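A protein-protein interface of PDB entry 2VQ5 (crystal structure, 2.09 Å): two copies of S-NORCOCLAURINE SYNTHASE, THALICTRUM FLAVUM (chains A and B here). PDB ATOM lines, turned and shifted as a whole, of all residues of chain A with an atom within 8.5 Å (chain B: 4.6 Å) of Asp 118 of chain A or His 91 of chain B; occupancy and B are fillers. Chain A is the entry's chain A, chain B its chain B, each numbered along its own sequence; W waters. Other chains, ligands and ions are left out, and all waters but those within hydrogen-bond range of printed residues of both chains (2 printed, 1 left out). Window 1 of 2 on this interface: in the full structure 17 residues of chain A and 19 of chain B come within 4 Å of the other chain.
N of Gly 87 of chain B lies within hydrogen-bond range of OD1 of Asp 118 of chain A, at 2.8 Å.
The backbone carbonyl oxygen (O) of Asp 118 of chain A sits close to the backbone NH (N) of Phe 89 of chain B.
Of the printed residues of chain B, Phe 89 of chain A touches Phe 89.
Printed residues of chain B within 4 Å of Leu 117 of chain A: Gly 87.
Of the printed residues of chain B, Leu 119 of chain A touches Phe 89.
Ile 155 of chain A touches none of the printed residues of chain B.
Thr 83 of chain B touches none of the printed residues of chain A.
Printed residues of chain A within 4 Å of Pro 86 of chain B: Asp 118.
Of the printed residues of chain A, Glu 88 of chain B touches Asp 118.
His 91 of chain B touches just one residue of chain A: Asp 118.
The nearest printed residue of chain B that does not touch Asp 118 of chain A is Pro 90 of chain B (5.9 Å).
The nearest residue of chain A that does not touch His 91 of chain B is Glu 92 of chain A (5.2 Å).
O of His 91 of chain B is in hydrogen-bond range of N of Phe 84 of chain B.
Water W2 lies within hydrogen-bond range of the backbone carbonyl oxygen of Asp 118 of chain A (2.7 Å), the backbone carbonyl oxygen of Gly 87 of chain B (3.0 Å) and the backbone NH of Phe 89 of chain B (3.5 Å).
Water W1 bridges ND1 of His 91 of chain B (3.2 Å) and OD2 of Asp 118 of chain A (3.4 Å).
Of the 10 printed residues of chain B, 5 touch a printed residue of chain A.
Hydrophobic or aromatic side chains of chain B within 4 Å of the printed part of chain A: Phe 89 and His 91.
Printed residues of chain A that touch a printed residue of chain B: Phe 89, Leu 117, Asp 118 and Leu 119.
Hydrophobic or aromatic side chains of chain A within 4 Å of the printed part of chain B: Phe 89 and Leu 119.
Among the printed residues, 8 pairs touch across the chains.
Phe 89 of chain A touches its own counterpart, Phe 89 of chain B.
3 positions are printed for both chains.
Phe 89 of chain A touches Phe 89 of chain B.
CA of Gly 87 of chain B touches O of Leu 117 of chain A, at 3.8 Å.
Asp 118 of chain A touches Pro 86 of chain B.
O of Glu 88 of chain B touches CB of Asp 118 of chain A, at 3.3 Å.
CB of His 91 of chain B touches OD2 of Asp 118 of chain A, 3.5 Å away.
Phe 89 of chain B touches Leu 119 of chain A.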
ATOM      1  N   PHE A  89      -8.427 -12.784 -25.400  1.00  0.00           N
ATOM      2  CA  PHE A  89      -7.162 -13.359 -24.921  1.00  0.00           C
ATOM      3  C   PHE A  89      -6.114 -12.272 -24.804  1.00  0.00           C
ATOM      4  O   PHE A  89      -6.043 -11.427 -25.686  1.00  0.00           O
ATOM      5  CB  PHE A  89      -6.651 -14.557 -25.709  1.00  0.00           C
ATOM      6  CG  PHE A  89      -5.512 -15.260 -25.023  1.00  0.00           C
ATOM      7  CD1 PHE A  89      -5.752 -16.103 -23.944  1.00  0.00           C
ATOM      8  CD2 PHE A  89      -4.196 -15.054 -25.433  1.00  0.00           C
ATOM      9  CE1 PHE A  89      -4.705 -16.739 -23.297  1.00  0.00           C
ATOM     10  CE2 PHE A  89      -3.151 -15.677 -24.791  1.00  0.00           C
ATOM     11  CZ  PHE A  89      -3.401 -16.519 -23.716  1.00  0.00           C
ATOM     12  N   HIS A  91      -6.838 -12.986 -20.965  1.00  0.00           N
ATOM     13  CA  HIS A  91      -7.895 -12.631 -20.035  1.00  0.00           C
ATOM     14  C   HIS A  91      -7.330 -11.797 -18.874  1.00  0.00           C
ATOM     15  O   HIS A  91      -7.972 -10.852 -18.422  1.00  0.00           O
ATOM     16  CB  HIS A  91      -8.631 -13.864 -19.502  1.00  0.00           C
ATOM     17  CG  HIS A  91      -9.563 -13.540 -18.380  1.00  0.00           C
ATOM     18  ND1 HIS A  91     -10.681 -12.753 -18.556  1.00  0.00           N
ATOM     19  CD2 HIS A  91      -9.500 -13.815 -17.057  1.00  0.00           C
ATOM     20  CE1 HIS A  91     -11.287 -12.586 -17.395  1.00  0.00           C
ATOM     21  NE2 HIS A  91     -10.597 -13.227 -16.470  1.00  0.00           N
ATOM     22  N   GLU A  92      -6.137 -12.150 -18.394  1.00  0.00           N
ATOM     23  CA  GLU A  92      -5.510 -11.434 -17.266  1.00  0.00           C
ATOM     24  C   GLU A  92      -3.994 -11.533 -17.257  1.00  0.00           C
ATOM     25  O   GLU A  92      -3.431 -12.591 -17.512  1.00  0.00           O
ATOM     26  CB  GLU A  92      -6.047 -11.939 -15.913  1.00  0.00           C
ATOM     27  CG  GLU A  92      -5.485 -11.190 -14.658  1.00  0.00           C
ATOM     28  CD  GLU A  92      -4.110 -11.704 -14.183  1.00  0.00           C
ATOM     29  OE1 GLU A  92      -3.742 -12.876 -14.459  1.00  0.00           O
ATOM     30  OE2 GLU A  92      -3.380 -10.939 -13.525  1.00  0.00           O
ATOM     31  N   TYR A  93      -3.351 -10.427 -16.908  1.00  0.00           N
ATOM     32  CA  TYR A  93      -1.919 -10.409 -16.646  1.00  0.00           C
ATOM     33  C   TYR A  93      -1.518  -9.212 -15.811  1.00  0.00           C
ATOM     34  O   TYR A  93      -2.276  -8.226 -15.700  1.00  0.00           O
ATOM     35  CB  TYR A  93      -1.088 -10.476 -17.941  1.00  0.00           C
ATOM     36  CG  TYR A  93      -1.327  -9.381 -18.961  1.00  0.00           C
ATOM     37  CD1 TYR A  93      -1.979  -9.660 -20.159  1.00  0.00           C
ATOM     38  CD2 TYR A  93      -0.864  -8.084 -18.751  1.00  0.00           C
ATOM     39  CE1 TYR A  93      -2.180  -8.666 -21.129  1.00  0.00           C
ATOM     40  CE2 TYR A  93      -1.064  -7.075 -19.720  1.00  0.00           C
ATOM     41  CZ  TYR A  93      -1.718  -7.376 -20.898  1.00  0.00           C
ATOM     42  OH  TYR A  93      -1.921  -6.395 -21.853  1.00  0.00           O
ATOM     43  N   LYS A  94      -0.326  -9.326 -15.224  1.00  0.00           N
ATOM     44  CA  LYS A  94       0.318  -8.264 -14.461  1.00  0.00           C
ATOM     45  C   LYS A  94       1.527  -7.735 -15.215  1.00  0.00           C
ATOM     46  O   LYS A  94       2.310  -8.506 -15.790  1.00  0.00           O
ATOM     47  CB  LYS A  94       0.784  -8.767 -13.100  1.00  0.00           C
ATOM     48  CG  LYS A  94      -0.325  -9.222 -12.150  1.00  0.00           C
ATOM     49  CD  LYS A  94       0.292  -9.867 -10.909  1.00  0.00           C
ATOM     50  CE  LYS A  94      -0.734 -10.124  -9.809  1.00  0.00           C
ATOM     51  NZ  LYS A  94      -1.803 -11.054 -10.276  1.00  0.00           N
ATOM     52  N   MET A 111       5.852  -7.694 -18.635  1.00  0.00           N
ATOM     53  CA  MET A 111       4.795  -8.603 -18.210  1.00  0.00           C
ATOM     54  C   MET A 111       5.388  -9.628 -17.252  1.00  0.00           C
ATOM     55  O   MET A 111       6.323 -10.363 -17.592  1.00  0.00           O
ATOM     56  CB  MET A 111       4.116  -9.298 -19.384  1.00  0.00           C
ATOM     57  CG  MET A 111       3.080 -10.307 -18.916  1.00  0.00           C
ATOM     58  SD  MET A 111       2.087 -11.118 -20.344  1.00  0.00           S
ATOM     59  CE  MET A 111       3.507 -12.039 -21.299  1.00  0.00           C
ATOM     60  N   ILE A 112       4.849  -9.662 -16.038  1.00  0.00           N
ATOM     61  CA  ILE A 112       5.470 -10.447 -14.965  1.00  0.00           C
ATOM     62  C   ILE A 112       4.712 -11.690 -14.527  1.00  0.00           C
ATOM     63  O   ILE A 112       5.310 -12.595 -13.924  1.00  0.00           O
ATOM     64  CB  ILE A 112       5.849  -9.566 -13.737  1.00  0.00           C
ATOM     65  CG1 ILE A 112       4.603  -8.892 -13.126  1.00  0.00           C
ATOM     66  CG2 ILE A 112       6.907  -8.531 -14.151  1.00  0.00           C
ATOM     67  CD1 ILE A 112       4.809  -8.329 -11.740  1.00  0.00           C
ATOM     68  N   GLU A 113       3.414 -11.741 -14.833  1.00  0.00           N
ATOM     69  CA  GLU A 113       2.576 -12.895 -14.484  1.00  0.00           C
ATOM     70  C   GLU A 113       1.369 -12.968 -15.421  1.00  0.00           C
ATOM     71  O   GLU A 113       0.842 -11.926 -15.839  1.00  0.00           O
ATOM     72  CB  GLU A 113       2.121 -12.799 -13.011  1.00  0.00           C
ATOM     73  CG  GLU A 113       1.386 -14.042 -12.489  1.00  0.00           C
ATOM     74  CD  GLU A 113       1.088 -14.014 -10.988  1.00  0.00           C
ATOM     75  OE1 GLU A 113       1.395 -13.008 -10.305  1.00  0.00           O
ATOM     76  OE2 GLU A 113       0.543 -15.027 -10.480  1.00  0.00           O
ATOM     77  N   GLY A 114       0.949 -14.188 -15.764  1.00  0.00           N
ATOM     78  CA  GLY A 114      -0.258 -14.413 -16.571  1.00  0.00           C
ATOM     79  C   GLY A 114      -0.071 -14.172 -18.057  1.00  0.00           C
ATOM     80  O   GLY A 114       1.053 -14.054 -18.526  1.00  0.00           O
ATOM     81  N   GLY A 115      -1.183 -14.087 -18.797  1.00  0.00           N
ATOM     82  CA  GLY A 115      -1.148 -13.891 -20.251  1.00  0.00           C
ATOM     83  C   GLY A 115      -0.241 -14.884 -20.975  1.00  0.00           C
ATOM     84  O   GLY A 115      -0.302 -16.091 -20.726  1.00  0.00           O
ATOM     85  N   TYR A 116       0.621 -14.364 -21.848  1.00  0.00           N
ATOM     86  CA  TYR A 116       1.521 -15.192 -22.670  1.00  0.00           C
ATOM     87  C   TYR A 116       2.522 -16.032 -21.875  1.00  0.00           C
ATOM     88  O   TYR A 116       3.023 -17.021 -22.390  1.00  0.00           O
ATOM     89  CB  TYR A 116       2.235 -14.353 -23.750  1.00  0.00           C
ATOM     90  CG  TYR A 116       1.273 -13.465 -24.524  1.00  0.00           C
ATOM     91  CD1 TYR A 116       0.343 -14.008 -25.401  1.00  0.00           C
ATOM     92  CD2 TYR A 116       1.270 -12.086 -24.340  1.00  0.00           C
ATOM     93  CE1 TYR A 116      -0.571 -13.201 -26.081  1.00  0.00           C
ATOM     94  CE2 TYR A 116       0.367 -11.267 -25.028  1.00  0.00           C
ATOM     95  CZ  TYR A 116      -0.540 -11.835 -25.895  1.00  0.00           C
ATOM     96  OH  TYR A 116      -1.431 -11.032 -26.575  1.00  0.00           O
ATOM     97  N   LEU A 117       2.789 -15.653 -20.626  1.00  0.00           N
ATOM     98  CA  LEU A 117       3.689 -16.418 -19.760  1.00  0.00           C
ATOM     99  C   LEU A 117       3.149 -17.802 -19.392  1.00  0.00           C
ATOM    100  O   LEU A 117       3.872 -18.625 -18.831  1.00  0.00           O
ATOM    101  CB  LEU A 117       4.041 -15.645 -18.492  1.00  0.00           C
ATOM    102  CG  LEU A 117       4.647 -14.244 -18.609  1.00  0.00           C
ATOM    103  CD1 LEU A 117       5.030 -13.748 -17.229  1.00  0.00           C
ATOM    104  CD2 LEU A 117       5.861 -14.235 -19.516  1.00  0.00           C
ATOM    105  N   ASP A 118       1.878 -18.044 -19.705  1.00  0.00           N
ATOM    106  CA  ASP A 118       1.259 -19.343 -19.485  1.00  0.00           C
ATOM    107  C   ASP A 118       1.192 -20.134 -20.784  1.00  0.00           C
ATOM    108  O   ASP A 118       0.717 -21.268 -20.804  1.00  0.00           O
ATOM    109  CB  ASP A 118      -0.145 -19.162 -18.910  1.00  0.00           C
ATOM    110  CG  ASP A 118      -0.128 -18.678 -17.477  1.00  0.00           C
ATOM    111  OD1 ASP A 118       0.892 -18.873 -16.781  1.00  0.00           O
ATOM    112  OD2 ASP A 118      -1.146 -18.109 -17.030  1.00  0.00           O
ATOM    113  N   LEU A 119       1.673 -19.526 -21.863  1.00  0.00           N
ATOM    114  CA  LEU A 119       1.630 -20.133 -23.190  1.00  0.00           C
ATOM    115  C   LEU A 119       3.046 -20.255 -23.794  1.00  0.00           C
ATOM    116  O   LEU A 119       3.258 -20.000 -24.988  1.00  0.00           O
ATOM    117  CB  LEU A 119       0.680 -19.322 -24.088  1.00  0.00           C
ATOM    118  CG  LEU A 119      -0.297 -20.003 -25.053  1.00  0.00           C
ATOM    119  CD1 LEU A 119      -0.856 -21.312 -24.527  1.00  0.00           C
ATOM    120  CD2 LEU A 119      -1.435 -19.055 -25.415  1.00  0.00           C
ATOM    121  N   GLY A 120       4.017 -20.616 -22.959  1.00  0.00           N
ATOM    122  CA  GLY A 120       5.363 -20.913 -23.447  1.00  0.00           C
ATOM    123  C   GLY A 120       6.354 -19.762 -23.482  1.00  0.00           C
ATOM    124  O   GLY A 120       7.513 -19.943 -23.906  1.00  0.00           O
ATOM    125  N   VAL A 121       5.912 -18.582 -23.031  1.00  0.00           N
ATOM    126  CA  VAL A 121       6.745 -17.385 -23.039  1.00  0.00           C
ATOM    127  C   VAL A 121       7.386 -17.246 -21.665  1.00  0.00           C
ATOM    128  O   VAL A 121       6.702 -17.341 -20.649  1.00  0.00           O
ATOM    129  CB  VAL A 121       5.927 -16.103 -23.434  1.00  0.00           C
ATOM    130  CG1 VAL A 121       6.760 -14.830 -23.282  1.00  0.00           C
ATOM    131  CG2 VAL A 121       5.375 -16.222 -24.849  1.00  0.00           C
ATOM    132  N   THR A 122       8.700 -17.034 -21.637  1.00  0.00           N
ATOM    133  CA  THR A 122       9.429 -16.961 -20.380  1.00  0.00           C
ATOM    134  C   THR A 122       9.800 -15.538 -20.014  1.00  0.00           C
ATOM    135  O   THR A 122      10.242 -15.271 -18.890  1.00  0.00           O
ATOM    136  CB  THR A 122      10.752 -17.790 -20.442  1.00  0.00           C
ATOM    137  OG1 THR A 122      11.563 -17.310 -21.511  1.00  0.00           O
ATOM    138  CG2 THR A 122      10.457 -19.273 -20.685  1.00  0.00           C
ATOM    139  N   PHE A 152       6.140 -23.381 -29.135  1.00  0.00           N
ATOM    140  CA  PHE A 152       4.936 -22.574 -28.915  1.00  0.00           C
ATOM    141  C   PHE A 152       4.913 -21.373 -29.850  1.00  0.00           C
ATOM    142  O   PHE A 152       3.984 -20.562 -29.806  1.00  0.00           O
ATOM    143  CB  PHE A 152       4.844 -22.088 -27.459  1.00  0.00           C
ATOM    144  CG  PHE A 152       4.354 -23.127 -26.499  1.00  0.00           C
ATOM    145  CD1 PHE A 152       5.245 -24.001 -25.882  1.00  0.00           C
ATOM    146  CD2 PHE A 152       3.001 -23.227 -26.194  1.00  0.00           C
ATOM    147  CE1 PHE A 152       4.795 -24.967 -24.973  1.00  0.00           C
ATOM    148  CE2 PHE A 152       2.539 -24.194 -25.296  1.00  0.00           C
ATOM    149  CZ  PHE A 152       3.443 -25.064 -24.682  1.00  0.00           C
ATOM    150  N   ILE A 155       1.760 -21.454 -31.866  1.00  0.00           N
ATOM    151  CA  ILE A 155       0.625 -21.069 -31.022  1.00  0.00           C
ATOM    152  C   ILE A 155       0.551 -19.569 -30.766  1.00  0.00           C
ATOM    153  O   ILE A 155      -0.478 -18.941 -31.015  1.00  0.00           O
ATOM    154  CB  ILE A 155       0.674 -21.750 -29.618  1.00  0.00           C
ATOM    155  CG1 ILE A 155       0.955 -23.259 -29.712  1.00  0.00           C
ATOM    156  CG2 ILE A 155      -0.602 -21.430 -28.812  1.00  0.00           C
ATOM    157  CD1 ILE A 155      -0.111 -24.064 -30.407  1.00  0.00           C
ATOM    158  N   VAL A 156       1.652 -19.007 -30.273  1.00  0.00           N
ATOM    159  CA  VAL A 156       1.629 -17.724 -29.579  1.00  0.00           C
ATOM    160  C   VAL A 156       1.893 -16.497 -30.464  1.00  0.00           C
ATOM    161  O   VAL A 156       1.452 -15.395 -30.131  1.00  0.00           O
ATOM    162  CB  VAL A 156       2.569 -17.763 -28.328  1.00  0.00           C
ATOM    163  CG1 VAL A 156       3.995 -17.311 -28.679  1.00  0.00           C
ATOM    164  CG2 VAL A 156       1.997 -16.939 -27.191  1.00  0.00           C
ATOM    165  N   MET B  82     -11.549 -23.899 -11.572  1.00  0.00           N
ATOM    166  CA  MET B  82     -10.232 -24.526 -11.492  1.00  0.00           C
ATOM    167  C   MET B  82      -9.123 -23.552 -11.871  1.00  0.00           C
ATOM    168  O   MET B  82      -9.122 -23.023 -12.986  1.00  0.00           O
ATOM    169  CB  MET B  82     -10.178 -25.733 -12.436  1.00  0.00           C
ATOM    170  CG  MET B  82     -11.151 -26.829 -12.064  1.00  0.00           C
ATOM    171  SD  MET B  82     -11.336 -28.271 -13.364  1.00  0.00           S
ATOM    172  CE  MET B  82     -11.986 -29.592 -12.084  1.00  0.00           C
ATOM    173  N   THR B  83      -8.179 -23.339 -10.953  1.00  0.00           N
ATOM    174  CA  THR B  83      -7.013 -22.492 -11.210  1.00  0.00           C
ATOM    175  C   THR B  83      -5.752 -23.366 -11.189  1.00  0.00           C
ATOM    176  O   THR B  83      -5.547 -24.157 -10.271  1.00  0.00           O
ATOM    177  CB  THR B  83      -6.907 -21.343 -10.169  1.00  0.00           C
ATOM    178  OG1 THR B  83      -8.170 -20.677 -10.072  1.00  0.00           O
ATOM    179  CG2 THR B  83      -5.820 -20.322 -10.561  1.00  0.00           C
ATOM    180  N   PHE B  84      -4.912 -23.216 -12.206  1.00  0.00           N
ATOM    181  CA  PHE B  84      -3.709 -24.036 -12.343  1.00  0.00           C
ATOM    182  C   PHE B  84      -2.436 -23.246 -12.022  1.00  0.00           C
ATOM    183  O   PHE B  84      -2.466 -22.015 -11.944  1.00  0.00           O
ATOM    184  CB  PHE B  84      -3.678 -24.664 -13.735  1.00  0.00           C
ATOM    185  CG  PHE B  84      -4.924 -25.449 -14.055  1.00  0.00           C
ATOM    186  CD1 PHE B  84      -5.016 -26.797 -13.721  1.00  0.00           C
ATOM    187  CD2 PHE B  84      -6.020 -24.827 -14.655  1.00  0.00           C
ATOM    188  CE1 PHE B  84      -6.175 -27.524 -13.999  1.00  0.00           C
ATOM    189  CE2 PHE B  84      -7.182 -25.534 -14.930  1.00  0.00           C
ATOM    190  CZ  PHE B  84      -7.265 -26.892 -14.600  1.00  0.00           C
ATOM    191  N   PRO B  86       1.234 -21.322 -12.192  1.00  0.00           N
ATOM    192  CA  PRO B  86       1.779 -20.453 -13.239  1.00  0.00           C
ATOM    193  C   PRO B  86       2.572 -21.251 -14.282  1.00  0.00           C
ATOM    194  O   PRO B  86       3.302 -22.182 -13.932  1.00  0.00           O
ATOM    195  CB  PRO B  86       2.700 -19.498 -12.456  1.00  0.00           C
ATOM    196  CG  PRO B  86       2.094 -19.468 -11.075  1.00  0.00           C
ATOM    197  CD  PRO B  86       1.636 -20.870 -10.841  1.00  0.00           C
ATOM    198  N   GLY B  87       2.389 -20.910 -15.555  1.00  0.00           N
ATOM    199  CA  GLY B  87       3.073 -21.590 -16.645  1.00  0.00           C
ATOM    200  C   GLY B  87       2.149 -22.485 -17.446  1.00  0.00           C
ATOM    201  O   GLY B  87       2.415 -22.783 -18.609  1.00  0.00           O
ATOM    202  N   GLU B  88       1.051 -22.914 -16.829  1.00  0.00           N
ATOM    203  CA  GLU B  88       0.127 -23.850 -17.474  1.00  0.00           C
ATOM    204  C   GLU B  88      -0.930 -23.084 -18.253  1.00  0.00           C
ATOM    205  O   GLU B  88      -1.343 -21.995 -17.839  1.00  0.00           O
ATOM    206  CB  GLU B  88      -0.559 -24.769 -16.442  1.00  0.00           C
ATOM    207  CG  GLU B  88       0.379 -25.424 -15.437  1.00  0.00           C
ATOM    208  CD  GLU B  88       1.351 -26.403 -16.080  1.00  0.00           C
ATOM    209  OE1 GLU B  88       2.522 -26.476 -15.626  1.00  0.00           O
ATOM    210  OE2 GLU B  88       0.944 -27.102 -17.041  1.00  0.00           O
ATOM    211  N   PHE B  89      -1.347 -23.656 -19.386  1.00  0.00           N
ATOM    212  CA  PHE B  89      -2.522 -23.169 -20.108  1.00  0.00           C
ATOM    213  C   PHE B  89      -3.625 -24.213 -20.004  1.00  0.00           C
ATOM    214  O   PHE B  89      -3.336 -25.371 -20.226  1.00  0.00           O
ATOM    215  CB  PHE B  89      -2.272 -22.655 -21.526  1.00  0.00           C
ATOM    216  CG  PHE B  89      -3.412 -21.834 -22.032  1.00  0.00           C
ATOM    217  CD1 PHE B  89      -3.547 -20.511 -21.643  1.00  0.00           C
ATOM    218  CD2 PHE B  89      -4.412 -22.415 -22.810  1.00  0.00           C
ATOM    219  CE1 PHE B  89      -4.630 -19.766 -22.050  1.00  0.00           C
ATOM    220  CE2 PHE B  89      -5.510 -21.678 -23.221  1.00  0.00           C
ATOM    221  CZ  PHE B  89      -5.620 -20.350 -22.848  1.00  0.00           C
ATOM    222  N   PRO B  90      -4.882 -23.761 -20.064  1.00  0.00           N
ATOM    223  CA  PRO B  90      -5.637 -22.888 -19.184  1.00  0.00           C
ATOM    224  C   PRO B  90      -4.998 -22.553 -17.847  1.00  0.00           C
ATOM    225  O   PRO B  90      -4.492 -23.430 -17.158  1.00  0.00           O
ATOM    226  CB  PRO B  90      -7.001 -23.560 -19.091  1.00  0.00           C
ATOM    227  CG  PRO B  90      -7.191 -24.099 -20.454  1.00  0.00           C
ATOM    228  CD  PRO B  90      -5.800 -24.586 -20.874  1.00  0.00           C
ATOM    229  N   HIS B  91      -4.987 -21.259 -17.521  1.00  0.00           N
ATOM    230  CA  HIS B  91      -4.691 -20.823 -16.163  1.00  0.00           C
ATOM    231  C   HIS B  91      -5.912 -21.032 -15.269  1.00  0.00           C
ATOM    232  O   HIS B  91      -5.779 -21.418 -14.120  1.00  0.00           O
ATOM    233  CB  HIS B  91      -4.254 -19.348 -16.124  1.00  0.00           C
ATOM    234  CG  HIS B  91      -4.132 -18.809 -14.733  1.00  0.00           C
ATOM    235  ND1 HIS B  91      -3.192 -19.276 -13.839  1.00  0.00           N
ATOM    236  CD2 HIS B  91      -4.882 -17.909 -14.054  1.00  0.00           C
ATOM    237  CE1 HIS B  91      -3.337 -18.653 -12.682  1.00  0.00           C
ATOM    238  NE2 HIS B  91      -4.357 -17.820 -12.785  1.00  0.00           N
ATOM    239  N   GLU B  92      -7.103 -20.764 -15.810  1.00  0.00           N
ATOM    240  CA  GLU B  92      -8.342 -20.810 -15.039  1.00  0.00           C
ATOM    241  C   GLU B  92      -9.555 -20.958 -15.959  1.00  0.00           C
ATOM    242  O   GLU B  92      -9.638 -20.300 -17.010  1.00  0.00           O
ATOM    243  CB  GLU B  92      -8.490 -19.553 -14.157  1.00  0.00           C
ATOM    244  CG  GLU B  92      -9.634 -19.645 -13.139  1.00  0.00           C
ATOM    245  CD  GLU B  92      -9.727 -18.442 -12.191  1.00  0.00           C
ATOM    246  OE1 GLU B  92      -9.136 -17.374 -12.491  1.00  0.00           O
ATOM    247  OE2 GLU B  92     -10.409 -18.566 -11.147  1.00  0.00           O
HETATM  248  O   HOH W   1      -0.605 -17.388 -13.711  1.00  0.00           O
HETATM  249  O   HOH W   2       1.565 -23.782 -21.284  1.00  0.00           O
